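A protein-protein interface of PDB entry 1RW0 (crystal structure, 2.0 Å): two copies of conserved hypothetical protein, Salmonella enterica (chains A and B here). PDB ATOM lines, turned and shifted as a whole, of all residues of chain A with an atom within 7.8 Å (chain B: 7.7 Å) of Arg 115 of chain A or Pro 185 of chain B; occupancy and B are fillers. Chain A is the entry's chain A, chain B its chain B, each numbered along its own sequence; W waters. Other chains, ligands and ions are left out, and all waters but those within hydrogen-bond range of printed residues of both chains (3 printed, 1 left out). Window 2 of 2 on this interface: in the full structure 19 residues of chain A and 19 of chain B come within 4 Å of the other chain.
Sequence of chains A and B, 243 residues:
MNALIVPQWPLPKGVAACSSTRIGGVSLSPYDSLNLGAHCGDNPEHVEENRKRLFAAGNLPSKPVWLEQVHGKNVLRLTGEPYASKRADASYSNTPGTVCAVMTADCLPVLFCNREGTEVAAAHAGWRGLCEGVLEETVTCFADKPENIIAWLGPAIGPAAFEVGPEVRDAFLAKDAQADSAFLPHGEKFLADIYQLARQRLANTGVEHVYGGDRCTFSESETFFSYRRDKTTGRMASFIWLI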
ATOM      1  N   PRO A  10     -27.546  -9.284 -33.449  1.00  0.00           N
ATOM      2  CA  PRO A  10     -27.492  -7.983 -32.777  1.00  0.00           C
ATOM      3  C   PRO A  10     -26.698  -7.009 -33.632  1.00  0.00           C
ATOM      4  O   PRO A  10     -25.633  -6.539 -33.235  1.00  0.00           O
ATOM      5  CB  PRO A  10     -26.782  -8.302 -31.465  1.00  0.00           C
ATOM      6  CG  PRO A  10     -27.116  -9.746 -31.234  1.00  0.00           C
ATOM      7  CD  PRO A  10     -26.951 -10.329 -32.602  1.00  0.00           C
ATOM      8  N   LEU A  11     -27.229  -6.720 -34.811  1.00  0.00           N
ATOM      9  CA  LEU A  11     -26.588  -5.826 -35.766  1.00  0.00           C
ATOM     10  C   LEU A  11     -26.473  -4.404 -35.217  1.00  0.00           C
ATOM     11  O   LEU A  11     -27.473  -3.790 -34.850  1.00  0.00           O
ATOM     12  CB  LEU A  11     -27.405  -5.824 -37.065  1.00  0.00           C
ATOM     13  CG  LEU A  11     -26.854  -5.203 -38.344  1.00  0.00           C
ATOM     14  CD1 LEU A  11     -25.743  -6.056 -38.902  1.00  0.00           C
ATOM     15  CD2 LEU A  11     -27.978  -5.088 -39.358  1.00  0.00           C
ATOM     16  N   PRO A  12     -25.242  -3.869 -35.129  1.00  0.00           N
ATOM     17  CA  PRO A  12     -25.096  -2.502 -34.617  1.00  0.00           C
ATOM     18  C   PRO A  12     -25.742  -1.482 -35.554  1.00  0.00           C
ATOM     19  O   PRO A  12     -25.906  -1.735 -36.745  1.00  0.00           O
ATOM     20  CB  PRO A  12     -23.578  -2.333 -34.497  1.00  0.00           C
ATOM     21  CG  PRO A  12     -23.033  -3.315 -35.489  1.00  0.00           C
ATOM     22  CD  PRO A  12     -23.927  -4.504 -35.312  1.00  0.00           C
ATOM     23  N   LYS A  13     -26.099  -0.331 -34.994  1.00  0.00           N
ATOM     24  CA  LYS A  13     -26.763   0.762 -35.706  1.00  0.00           C
ATOM     25  C   LYS A  13     -26.434   1.078 -37.173  1.00  0.00           C
ATOM     26  O   LYS A  13     -27.319   1.027 -38.032  1.00  0.00           O
ATOM     27  CB  LYS A  13     -26.617   2.056 -34.896  1.00  0.00           C
ATOM     28  CG  LYS A  13     -27.300   2.020 -33.537  1.00  0.00           C
ATOM     29  CD  LYS A  13     -27.167   3.358 -32.820  1.00  0.00           C
ATOM     30  CE  LYS A  13     -27.915   3.355 -31.499  1.00  0.00           C
ATOM     31  NZ  LYS A  13     -29.372   3.091 -31.689  1.00  0.00           N
ATOM     32  N   GLY A  14     -25.183   1.418 -37.462  1.00  0.00           N
ATOM     33  CA  GLY A  14     -24.831   1.789 -38.826  1.00  0.00           C
ATOM     34  C   GLY A  14     -24.376   0.709 -39.789  1.00  0.00           C
ATOM     35  O   GLY A  14     -23.601   0.984 -40.708  1.00  0.00           O
ATOM     36  N   VAL A  15     -24.863  -0.512 -39.600  1.00  0.00           N
ATOM     37  CA  VAL A  15     -24.476  -1.620 -40.469  1.00  0.00           C
ATOM     38  C   VAL A  15     -25.709  -2.274 -41.099  1.00  0.00           C
ATOM     39  O   VAL A  15     -26.795  -2.256 -40.524  1.00  0.00           O
ATOM     40  CB  VAL A  15     -23.686  -2.693 -39.671  1.00  0.00           C
ATOM     41  CG1 VAL A  15     -23.219  -3.810 -40.595  1.00  0.00           C
ATOM     42  CG2 VAL A  15     -22.491  -2.051 -38.962  1.00  0.00           C
ATOM     43  N   CYS A 113     -18.608  -7.722 -38.354  1.00  0.00           N
ATOM     44  CA  CYS A 113     -18.729  -6.304 -38.052  1.00  0.00           C
ATOM     45  C   CYS A 113     -18.407  -6.155 -36.572  1.00  0.00           C
ATOM     46  O   CYS A 113     -18.573  -7.103 -35.807  1.00  0.00           O
ATOM     47  CB  CYS A 113     -20.134  -5.777 -38.364  1.00  0.00           C
ATOM     48  SG  CYS A 113     -21.415  -6.214 -37.189  1.00  0.00           S
ATOM     49  N   ASN A 114     -17.915  -4.988 -36.169  1.00  0.00           N
ATOM     50  CA  ASN A 114     -17.603  -4.775 -34.760  1.00  0.00           C
ATOM     51  C   ASN A 114     -18.824  -4.160 -34.079  1.00  0.00           C
ATOM     52  O   ASN A 114     -19.722  -3.647 -34.744  1.00  0.00           O
ATOM     53  CB  ASN A 114     -16.357  -3.885 -34.606  1.00  0.00           C
ATOM     54  CG  ASN A 114     -16.530  -2.514 -35.224  1.00  0.00           C
ATOM     55  OD1 ASN A 114     -17.373  -2.314 -36.092  1.00  0.00           O
ATOM     56  ND2 ASN A 114     -15.713  -1.560 -34.785  1.00  0.00           N
ATOM     57  N   ARG A 115     -18.864  -4.229 -32.755  1.00  0.00           N
ATOM     58  CA  ARG A 115     -19.998  -3.704 -32.009  1.00  0.00           C
ATOM     59  C   ARG A 115     -20.215  -2.214 -32.233  1.00  0.00           C
ATOM     60  O   ARG A 115     -21.350  -1.742 -32.189  1.00  0.00           O
ATOM     61  CB  ARG A 115     -19.818  -3.995 -30.519  1.00  0.00           C
ATOM     62  CG  ARG A 115     -19.819  -5.481 -30.191  1.00  0.00           C
ATOM     63  CD  ARG A 115     -19.250  -5.730 -28.811  1.00  0.00           C
ATOM     64  NE  ARG A 115     -20.015  -5.031 -27.785  1.00  0.00           N
ATOM     65  CZ  ARG A 115     -19.495  -4.575 -26.651  1.00  0.00           C
ATOM     66  NH1 ARG A 115     -18.201  -4.746 -26.399  1.00  0.00           N
ATOM     67  NH2 ARG A 115     -20.266  -3.946 -25.776  1.00  0.00           N
ATOM     68  N   GLU A 116     -19.130  -1.480 -32.484  1.00  0.00           N
ATOM     69  CA  GLU A 116     -19.220  -0.039 -32.713  1.00  0.00           C
ATOM     70  C   GLU A 116     -19.761   0.299 -34.098  1.00  0.00           C
ATOM     71  O   GLU A 116     -20.067   1.460 -34.386  1.00  0.00           O
ATOM     72  CB  GLU A 116     -17.848   0.611 -32.528  1.00  0.00           C
ATOM     73  CG  GLU A 116     -17.307   0.455 -31.127  1.00  0.00           C
ATOM     74  CD  GLU A 116     -18.276   0.973 -30.091  1.00  0.00           C
ATOM     75  OE1 GLU A 116     -18.492   2.203 -30.055  1.00  0.00           O
ATOM     76  OE2 GLU A 116     -18.829   0.149 -29.327  1.00  0.00           O
ATOM     77  N   GLY A 117     -19.879  -0.711 -34.956  1.00  0.00           N
ATOM     78  CA  GLY A 117     -20.395  -0.485 -36.297  1.00  0.00           C
ATOM     79  C   GLY A 117     -19.519   0.421 -37.143  1.00  0.00           C
ATOM     80  O   GLY A 117     -20.010   1.338 -37.801  1.00  0.00           O
ATOM     81  N   THR A 118     -18.217   0.161 -37.137  1.00  0.00           N
ATOM     82  CA  THR A 118     -17.283   0.966 -37.908  1.00  0.00           C
ATOM     83  C   THR A 118     -16.424   0.125 -38.844  1.00  0.00           C
ATOM     84  O   THR A 118     -15.650   0.667 -39.629  1.00  0.00           O
ATOM     85  CB  THR A 118     -16.353   1.766 -36.979  1.00  0.00           C
ATOM     86  OG1 THR A 118     -15.617   0.858 -36.148  1.00  0.00           O
ATOM     87  CG2 THR A 118     -17.168   2.707 -36.094  1.00  0.00           C
ATOM     88  N   GLU A 119     -16.542  -1.196 -38.751  1.00  0.00           N
ATOM     89  CA  GLU A 119     -15.767  -2.085 -39.622  1.00  0.00           C
ATOM     90  C   GLU A 119     -16.616  -3.295 -39.986  1.00  0.00           C
ATOM     91  O   GLU A 119     -17.331  -3.834 -39.139  1.00  0.00           O
ATOM     92  CB  GLU A 119     -14.496  -2.601 -38.927  1.00  0.00           C
ATOM     93  CG  GLU A 119     -13.670  -1.583 -38.170  1.00  0.00           C
ATOM     94  CD  GLU A 119     -12.448  -2.214 -37.514  1.00  0.00           C
ATOM     95  OE1 GLU A 119     -11.503  -2.597 -38.241  1.00  0.00           O
ATOM     96  OE2 GLU A 119     -12.435  -2.340 -36.272  1.00  0.00           O
ATOM     97  N   PHE A 142      -9.197  -6.505 -38.785  1.00  0.00           N
ATOM     98  CA  PHE A 142      -9.921  -5.559 -37.951  1.00  0.00           C
ATOM     99  C   PHE A 142      -8.991  -4.822 -36.999  1.00  0.00           C
ATOM    100  O   PHE A 142      -8.045  -5.405 -36.466  1.00  0.00           O
ATOM    101  CB  PHE A 142     -10.999  -6.278 -37.139  1.00  0.00           C
ATOM    102  CG  PHE A 142     -12.251  -6.574 -37.916  1.00  0.00           C
ATOM    103  CD1 PHE A 142     -13.405  -5.826 -37.709  1.00  0.00           C
ATOM    104  CD2 PHE A 142     -12.282  -7.615 -38.839  1.00  0.00           C
ATOM    105  CE1 PHE A 142     -14.582  -6.109 -38.410  1.00  0.00           C
ATOM    106  CE2 PHE A 142     -13.457  -7.910 -39.548  1.00  0.00           C
ATOM    107  CZ  PHE A 142     -14.606  -7.154 -39.331  1.00  0.00           C
ATOM    108  N   ASP A 144     -10.288  -3.331 -34.383  1.00  0.00           N
ATOM    109  CA  ASP A 144     -10.931  -3.618 -33.103  1.00  0.00           C
ATOM    110  C   ASP A 144     -10.458  -4.960 -32.556  1.00  0.00           C
ATOM    111  O   ASP A 144      -9.906  -5.779 -33.286  1.00  0.00           O
ATOM    112  CB  ASP A 144     -12.453  -3.650 -33.272  1.00  0.00           C
ATOM    113  CG  ASP A 144     -13.189  -3.103 -32.063  1.00  0.00           C
ATOM    114  OD1 ASP A 144     -12.780  -3.398 -30.918  1.00  0.00           O
ATOM    115  OD2 ASP A 144     -14.191  -2.382 -32.263  1.00  0.00           O
ATOM    116  N   LYS A 145     -10.675  -5.184 -31.267  1.00  0.00           N
ATOM    117  CA  LYS A 145     -10.273  -6.439 -30.647  1.00  0.00           C
ATOM    118  C   LYS A 145     -11.272  -7.525 -31.036  1.00  0.00           C
ATOM    119  O   LYS A 145     -12.461  -7.254 -31.181  1.00  0.00           O
ATOM    120  CB  LYS A 145     -10.240  -6.285 -29.127  1.00  0.00           C
ATOM    121  CG  LYS A 145      -9.249  -5.226 -28.638  1.00  0.00           C
ATOM    122  CD  LYS A 145      -9.252  -5.097 -27.120  1.00  0.00           C
ATOM    123  CE  LYS A 145     -10.538  -4.482 -26.601  1.00  0.00           C
ATOM    124  NZ  LYS A 145     -11.727  -5.341 -26.850  1.00  0.00           N
ATOM    125  N   PRO A 146     -10.799  -8.769 -31.210  1.00  0.00           N
ATOM    126  CA  PRO A 146     -11.633  -9.915 -31.583  1.00  0.00           C
ATOM    127  C   PRO A 146     -12.916 -10.054 -30.767  1.00  0.00           C
ATOM    128  O   PRO A 146     -13.974 -10.351 -31.314  1.00  0.00           O
ATOM    129  CB  PRO A 146     -10.697 -11.101 -31.374  1.00  0.00           C
ATOM    130  CG  PRO A 146      -9.369 -10.533 -31.743  1.00  0.00           C
ATOM    131  CD  PRO A 146      -9.391  -9.180 -31.058  1.00  0.00           C
ATOM    132  N   GLU A 147     -12.814  -9.845 -29.459  1.00  0.00           N
ATOM    133  CA  GLU A 147     -13.971  -9.961 -28.573  1.00  0.00           C
ATOM    134  C   GLU A 147     -15.079  -8.973 -28.930  1.00  0.00           C
ATOM    135  O   GLU A 147     -16.236  -9.165 -28.546  1.00  0.00           O
ATOM    136  CB  GLU A 147     -13.550  -9.741 -27.116  1.00  0.00           C
ATOM    137  CG  GLU A 147     -13.230  -8.290 -26.774  1.00  0.00           C
ATOM    138  CD  GLU A 147     -12.757  -8.102 -25.338  1.00  0.00           C
ATOM    139  OE1 GLU A 147     -11.692  -8.654 -24.979  1.00  0.00           O
ATOM    140  OE2 GLU A 147     -13.448  -7.399 -24.569  1.00  0.00           O
ATOM    141  N   ASN A 148     -14.729  -7.909 -29.648  1.00  0.00           N
ATOM    142  CA  ASN A 148     -15.716  -6.906 -30.041  1.00  0.00           C
ATOM    143  C   ASN A 148     -16.247  -7.141 -31.446  1.00  0.00           C
ATOM    144  O   ASN A 148     -16.979  -6.312 -31.992  1.00  0.00           O
ATOM    145  CB  ASN A 148     -15.119  -5.497 -29.967  1.00  0.00           C
ATOM    146  CG  ASN A 148     -14.881  -5.037 -28.543  1.00  0.00           C
ATOM    147  OD1 ASN A 148     -15.709  -5.261 -27.655  1.00  0.00           O
ATOM    148  ND2 ASN A 148     -13.754  -4.368 -28.321  1.00  0.00           N
ATOM    149  N   ILE A 149     -15.875  -8.267 -32.038  1.00  0.00           N
ATOM    150  CA  ILE A 149     -16.326  -8.582 -33.383  1.00  0.00           C
ATOM    151  C   ILE A 149     -17.415  -9.645 -33.353  1.00  0.00           C
ATOM    152  O   ILE A 149     -17.241 -10.695 -32.738  1.00  0.00           O
ATOM    153  CB  ILE A 149     -15.161  -9.103 -34.250  1.00  0.00           C
ATOM    154  CG1 ILE A 149     -14.115  -7.996 -34.439  1.00  0.00           C
ATOM    155  CG2 ILE A 149     -15.695  -9.590 -35.597  1.00  0.00           C
ATOM    156  CD1 ILE A 149     -12.825  -8.475 -35.073  1.00  0.00           C
ATOM    157  N   ILE A 150     -18.538  -9.375 -34.009  1.00  0.00           N
ATOM    158  CA  ILE A 150     -19.608 -10.359 -34.058  1.00  0.00           C
ATOM    159  C   ILE A 150     -19.632 -10.936 -35.464  1.00  0.00           C
ATOM    160  O   ILE A 150     -19.239 -10.271 -36.432  1.00  0.00           O
ATOM    161  CB  ILE A 150     -20.991  -9.763 -33.697  1.00  0.00           C
ATOM    162  CG1 ILE A 150     -21.437  -8.752 -34.750  1.00  0.00           C
ATOM    163  CG2 ILE A 150     -20.924  -9.118 -32.323  1.00  0.00           C
ATOM    164  CD1 ILE A 150     -22.850  -8.218 -34.516  1.00  0.00           C
ATOM    165  N   GLU A 208     -16.189 -14.183 -29.781  1.00  0.00           N
ATOM    166  CA  GLU A 208     -17.145 -14.853 -28.903  1.00  0.00           C
ATOM    167  C   GLU A 208     -18.583 -14.912 -29.422  1.00  0.00           C
ATOM    168  O   GLU A 208     -19.280 -15.909 -29.234  1.00  0.00           O
ATOM    169  CB  GLU A 208     -17.152 -14.160 -27.535  1.00  0.00           C
ATOM    170  CG  GLU A 208     -15.784 -14.053 -26.876  1.00  0.00           C
ATOM    171  CD  GLU A 208     -15.826 -13.351 -25.524  1.00  0.00           C
ATOM    172  OE1 GLU A 208     -14.770 -13.277 -24.859  1.00  0.00           O
ATOM    173  OE2 GLU A 208     -16.911 -12.874 -25.122  1.00  0.00           O
ATOM    174  N   HIS A 209     -19.030 -13.848 -30.074  1.00  0.00           N
ATOM    175  CA  HIS A 209     -20.405 -13.790 -30.548  1.00  0.00           C
ATOM    176  C   HIS A 209     -20.579 -14.203 -32.003  1.00  0.00           C
ATOM    177  O   HIS A 209     -20.337 -13.417 -32.920  1.00  0.00           O
ATOM    178  CB  HIS A 209     -20.952 -12.384 -30.309  1.00  0.00           C
ATOM    179  CG  HIS A 209     -20.660 -11.860 -28.933  1.00  0.00           C
ATOM    180  ND1 HIS A 209     -21.076 -12.504 -27.787  1.00  0.00           N
ATOM    181  CD2 HIS A 209     -19.962 -10.775 -28.520  1.00  0.00           C
ATOM    182  CE1 HIS A 209     -20.647 -11.840 -26.728  1.00  0.00           C
ATOM    183  NE2 HIS A 209     -19.969 -10.786 -27.145  1.00  0.00           N
ATOM    184  N   TYR A 211     -23.336 -15.883 -34.717  1.00  0.00           N
ATOM    185  CA  TYR A 211     -24.764 -16.121 -34.952  1.00  0.00           C
ATOM    186  C   TYR A 211     -25.030 -16.876 -36.255  1.00  0.00           C
ATOM    187  O   TYR A 211     -24.110 -17.149 -37.022  1.00  0.00           O
ATOM    188  CB  TYR A 211     -25.494 -14.773 -34.982  1.00  0.00           C
ATOM    189  CG  TYR A 211     -25.230 -13.936 -33.751  1.00  0.00           C
ATOM    190  CD1 TYR A 211     -25.983 -14.112 -32.591  1.00  0.00           C
ATOM    191  CD2 TYR A 211     -24.190 -13.005 -33.727  1.00  0.00           C
ATOM    192  CE1 TYR A 211     -25.704 -13.385 -31.432  1.00  0.00           C
ATOM    193  CE2 TYR A 211     -23.902 -12.272 -32.572  1.00  0.00           C
ATOM    194  CZ  TYR A 211     -24.660 -12.469 -31.432  1.00  0.00           C
ATOM    195  OH  TYR A 211     -24.365 -11.774 -30.288  1.00  0.00           O
ATOM    196  N   ARG B 169     -27.074 -13.633 -16.349  1.00  0.00           N
ATOM    197  CA  ARG B 169     -25.664 -13.717 -16.699  1.00  0.00           C
ATOM    198  C   ARG B 169     -24.835 -14.161 -15.494  1.00  0.00           C
ATOM    199  O   ARG B 169     -23.986 -15.043 -15.616  1.00  0.00           O
ATOM    200  CB  ARG B 169     -25.150 -12.364 -17.204  1.00  0.00           C
ATOM    201  CG  ARG B 169     -23.643 -12.324 -17.426  1.00  0.00           C
ATOM    202  CD  ARG B 169     -23.224 -11.068 -18.185  1.00  0.00           C
ATOM    203  NE  ARG B 169     -21.774 -10.997 -18.355  1.00  0.00           N
ATOM    204  CZ  ARG B 169     -20.933 -10.508 -17.448  1.00  0.00           C
ATOM    205  NH1 ARG B 169     -21.390 -10.033 -16.299  1.00  0.00           N
ATOM    206  NH2 ARG B 169     -19.631 -10.501 -17.688  1.00  0.00           N
ATOM    207  N   ASP B 180     -19.592 -16.559 -20.223  1.00  0.00           N
ATOM    208  CA  ASP B 180     -19.624 -15.127 -20.492  1.00  0.00           C
ATOM    209  C   ASP B 180     -19.630 -14.817 -21.992  1.00  0.00           C
ATOM    210  O   ASP B 180     -20.079 -13.750 -22.408  1.00  0.00           O
ATOM    211  CB  ASP B 180     -18.434 -14.451 -19.805  1.00  0.00           C
ATOM    212  CG  ASP B 180     -18.508 -12.939 -19.863  1.00  0.00           C
ATOM    213  OD1 ASP B 180     -19.625 -12.392 -19.724  1.00  0.00           O
ATOM    214  OD2 ASP B 180     -17.449 -12.299 -20.033  1.00  0.00           O
ATOM    215  N   ALA B 182     -21.470 -16.073 -24.127  1.00  0.00           N
ATOM    216  CA  ALA B 182     -22.837 -16.144 -24.625  1.00  0.00           C
ATOM    217  C   ALA B 182     -23.689 -14.915 -24.312  1.00  0.00           C
ATOM    218  O   ALA B 182     -24.874 -14.877 -24.652  1.00  0.00           O
ATOM    219  CB  ALA B 182     -23.515 -17.392 -24.070  1.00  0.00           C
ATOM    220  N   PHE B 183     -23.090 -13.912 -23.674  1.00  0.00           N
ATOM    221  CA  PHE B 183     -23.824 -12.710 -23.303  1.00  0.00           C
ATOM    222  C   PHE B 183     -23.233 -11.461 -23.929  1.00  0.00           C
ATOM    223  O   PHE B 183     -22.079 -11.120 -23.680  1.00  0.00           O
ATOM    224  CB  PHE B 183     -23.838 -12.572 -21.777  1.00  0.00           C
ATOM    225  CG  PHE B 183     -24.529 -13.710 -21.075  1.00  0.00           C
ATOM    226  CD1 PHE B 183     -25.889 -13.636 -20.770  1.00  0.00           C
ATOM    227  CD2 PHE B 183     -23.833 -14.871 -20.761  1.00  0.00           C
ATOM    228  CE1 PHE B 183     -26.546 -14.705 -20.162  1.00  0.00           C
ATOM    229  CE2 PHE B 183     -24.479 -15.950 -20.152  1.00  0.00           C
ATOM    230  CZ  PHE B 183     -25.840 -15.867 -19.852  1.00  0.00           C
ATOM    231  N   LEU B 184     -24.026 -10.785 -24.753  1.00  0.00           N
ATOM    232  CA  LEU B 184     -23.577  -9.561 -25.407  1.00  0.00           C
ATOM    233  C   LEU B 184     -24.219  -8.385 -24.687  1.00  0.00           C
ATOM    234  O   LEU B 184     -25.435  -8.362 -24.489  1.00  0.00           O
ATOM    235  CB  LEU B 184     -23.994  -9.558 -26.883  1.00  0.00           C
ATOM    236  CG  LEU B 184     -23.730  -8.275 -27.679  1.00  0.00           C
ATOM    237  CD1 LEU B 184     -22.245  -8.105 -27.937  1.00  0.00           C
ATOM    238  CD2 LEU B 184     -24.483  -8.340 -29.000  1.00  0.00           C
ATOM    239  N   PRO B 185     -23.409  -7.395 -24.271  1.00  0.00           N
ATOM    240  CA  PRO B 185     -23.964  -6.233 -23.571  1.00  0.00           C
ATOM    241  C   PRO B 185     -25.024  -5.526 -24.405  1.00  0.00           C
ATOM    242  O   PRO B 185     -24.823  -5.261 -25.592  1.00  0.00           O
ATOM    243  CB  PRO B 185     -22.734  -5.360 -23.324  1.00  0.00           C
ATOM    244  CG  PRO B 185     -21.640  -6.365 -23.174  1.00  0.00           C
ATOM    245  CD  PRO B 185     -21.939  -7.328 -24.309  1.00  0.00           C
ATOM    246  N   HIS B 186     -26.155  -5.230 -23.779  1.00  0.00           N
ATOM    247  CA  HIS B 186     -27.258  -4.556 -24.450  1.00  0.00           C
ATOM    248  C   HIS B 186     -27.812  -3.539 -23.464  1.00  0.00           C
ATOM    249  O   HIS B 186     -28.710  -3.844 -22.678  1.00  0.00           O
ATOM    250  CB  HIS B 186     -28.340  -5.570 -24.831  1.00  0.00           C
ATOM    251  CG  HIS B 186     -29.404  -5.015 -25.726  1.00  0.00           C
ATOM    252  ND1 HIS B 186     -29.162  -4.648 -27.032  1.00  0.00           N
ATOM    253  CD2 HIS B 186     -30.715  -4.762 -25.501  1.00  0.00           C
ATOM    254  CE1 HIS B 186     -30.277  -4.194 -27.574  1.00  0.00           C
ATOM    255  NE2 HIS B 186     -31.236  -4.253 -26.666  1.00  0.00           N
ATOM    256  N   GLY B 187     -27.272  -2.327 -23.509  1.00  0.00           N
ATOM    257  CA  GLY B 187     -27.711  -1.302 -22.584  1.00  0.00           C
ATOM    258  C   GLY B 187     -27.328  -1.758 -21.192  1.00  0.00           C
ATOM    259  O   GLY B 187     -26.166  -2.081 -20.946  1.00  0.00           O
ATOM    260  N   GLU B 188     -28.301  -1.809 -20.286  1.00  0.00           N
ATOM    261  CA  GLU B 188     -28.048  -2.240 -18.914  1.00  0.00           C
ATOM    262  C   GLU B 188     -28.298  -3.747 -18.779  1.00  0.00           C
ATOM    263  O   GLU B 188     -28.124  -4.330 -17.706  1.00  0.00           O
ATOM    264  CB  GLU B 188     -28.963  -1.476 -17.953  1.00  0.00           C
ATOM    265  CG  GLU B 188     -28.395  -1.305 -16.557  1.00  0.00           C
ATOM    266  CD  GLU B 188     -27.122  -0.475 -16.547  1.00  0.00           C
ATOM    267  OE1 GLU B 188     -27.158   0.677 -17.039  1.00  0.00           O
ATOM    268  OE2 GLU B 188     -26.086  -0.970 -16.047  1.00  0.00           O
ATOM    269  N   LYS B 189     -28.704  -4.372 -19.878  1.00  0.00           N
ATOM    270  CA  LYS B 189     -28.979  -5.804 -19.894  1.00  0.00           C
ATOM    271  C   LYS B 189     -28.040  -6.546 -20.843  1.00  0.00           C
ATOM    272  O   LYS B 189     -26.977  -6.037 -21.208  1.00  0.00           O
ATOM    273  CB  LYS B 189     -30.435  -6.052 -20.303  1.00  0.00           C
ATOM    274  CG  LYS B 189     -31.457  -5.633 -19.256  1.00  0.00           C
ATOM    275  CD  LYS B 189     -32.868  -5.978 -19.703  1.00  0.00           C
ATOM    276  CE  LYS B 189     -33.853  -5.889 -18.549  1.00  0.00           C
ATOM    277  NZ  LYS B 189     -33.827  -4.550 -17.908  1.00  0.00           N
ATOM    278  N   PHE B 190     -28.435  -7.753 -21.235  1.00  0.00           N
ATOM    279  CA  PHE B 190     -27.623  -8.569 -22.133  1.00  0.00           C
ATOM    280  C   PHE B 190     -28.490  -9.358 -23.105  1.00  0.00           C
ATOM    281  O   PHE B 190     -29.653  -9.646 -22.823  1.00  0.00           O
ATOM    282  CB  PHE B 190     -26.785  -9.568 -21.326  1.00  0.00           C
ATOM    283  CG  PHE B 190     -25.788  -8.927 -20.403  1.00  0.00           C
ATOM    284  CD1 PHE B 190     -24.536  -8.535 -20.871  1.00  0.00           C
ATOM    285  CD2 PHE B 190     -26.102  -8.714 -19.065  1.00  0.00           C
ATOM    286  CE1 PHE B 190     -23.608  -7.938 -20.016  1.00  0.00           C
ATOM    287  CE2 PHE B 190     -25.183  -8.118 -18.203  1.00  0.00           C
ATOM    288  CZ  PHE B 190     -23.933  -7.731 -18.683  1.00  0.00           C
ATOM    289  N   LEU B 191     -27.917  -9.691 -24.256  1.00  0.00           N
ATOM    290  CA  LEU B 191     -28.602 -10.509 -25.250  1.00  0.00           C
ATOM    291  C   LEU B 191     -27.910 -11.855 -25.104  1.00  0.00           C
ATOM    292  O   LEU B 191     -26.718 -11.978 -25.386  1.00  0.00           O
ATOM    293  CB  LEU B 191     -28.401  -9.955 -26.666  1.00  0.00           C
ATOM    294  CG  LEU B 191     -29.191  -8.692 -27.025  1.00  0.00           C
ATOM    295  CD1 LEU B 191     -28.905  -8.295 -28.463  1.00  0.00           C
ATOM    296  CD2 LEU B 191     -30.681  -8.947 -26.835  1.00  0.00           C
ATOM    297  N   ALA B 192     -28.643 -12.863 -24.644  1.00  0.00           N
ATOM    298  CA  ALA B 192     -28.050 -14.180 -24.440  1.00  0.00           C
ATOM    299  C   ALA B 192     -28.359 -15.180 -25.550  1.00  0.00           C
ATOM    300  O   ALA B 192     -29.471 -15.224 -26.068  1.00  0.00           O
ATOM    301  CB  ALA B 192     -28.501 -14.741 -23.096  1.00  0.00           C
HETATM  302  O   HOH W   1     -26.525 -11.597 -28.835  1.00  0.00           O
HETATM  303  O   HOH W   2     -22.919  -4.773 -27.309  1.00  0.00           O
HETATM  304  O   HOH W   3     -25.362 -13.300 -27.321  1.00  0.00           O
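CD2 of Leu 184 of chain B touches CB of Pro 10 of chain A, at 3.4 Å.
CG of Pro 10 of chain A touches CD1 of Leu 191 of chain B (3.6 Å).
NE of Arg 115 of chain A touches CD1 of Leu 184 of chain B, at 3.8 Å.
Arg 115 of chain A touches Pro 185 of chain B.
O of Phe 183 of chain B touches CE1 of His 209 of chain A, at 3.4 Å.
CD2 of His 209 of chain A touches CD1 of Leu 184 of chain B (3.6 Å).
Tyr 211 of chain A touches Leu 184 of chain B (OH to CD2, 3.7 Å).
Pro 185 of chain B touches one residue of chain A.
Of the printed residues of chain A, Leu 191 of chain B touches Pro 10.
Of the printed residues of chain B, His 209 of chain A touches Phe 183 and Leu 184.
Printed residues of chain B within 4 Å of Tyr 211 of chain A: Leu 184.
Printed residues of chain A within 4 Å of Phe 183 of chain B: His 209 (3.4 Å).
Of the printed residues of chain B, Pro 10 of chain A touches Leu 184 and Leu 191.
The nearest residue of chain A that does not touch Pro 185 of chain B is His 209 of chain A (4.9 Å).
The nearest printed residue of chain B that does not touch His 209 of chain A is Asp 180 of chain B (4.8 Å).
NH1 of Arg 115 of chain A sits at hydrogen-bond distance from OD1 of Asn 148 of chain A (2.8 Å).
The backbone carbonyl oxygen (O) of Leu 184 of chain B lies within hydrogen-bond range of the backbone NH (N) of Leu 191 of chain B.
No position is printed for both chains.
Of the 13 printed residues of chain B, 4 touch a printed residue of chain A.
Among the printed residues, 7 pairs touch across the chains.
Water W1 bridges the side-chain hydroxyl (OH) of Tyr 211 of chain A and the backbone carbonyl oxygen (O) of Leu 191 of chain B.
Water W2 lies within hydrogen-bond range of O of Pro 185 of chain B (2.6 Å) and NE of Arg 115 of chain A (3.0 Å).
Water W3 lies within hydrogen-bond range of the backbone carbonyl oxygen of Leu 191 of chain B (2.7 Å), the backbone carbonyl oxygen of Ala 182 of chain B (3.1 Å) and the side-chain hydroxyl of Tyr 211 of chain A (3.5 Å).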
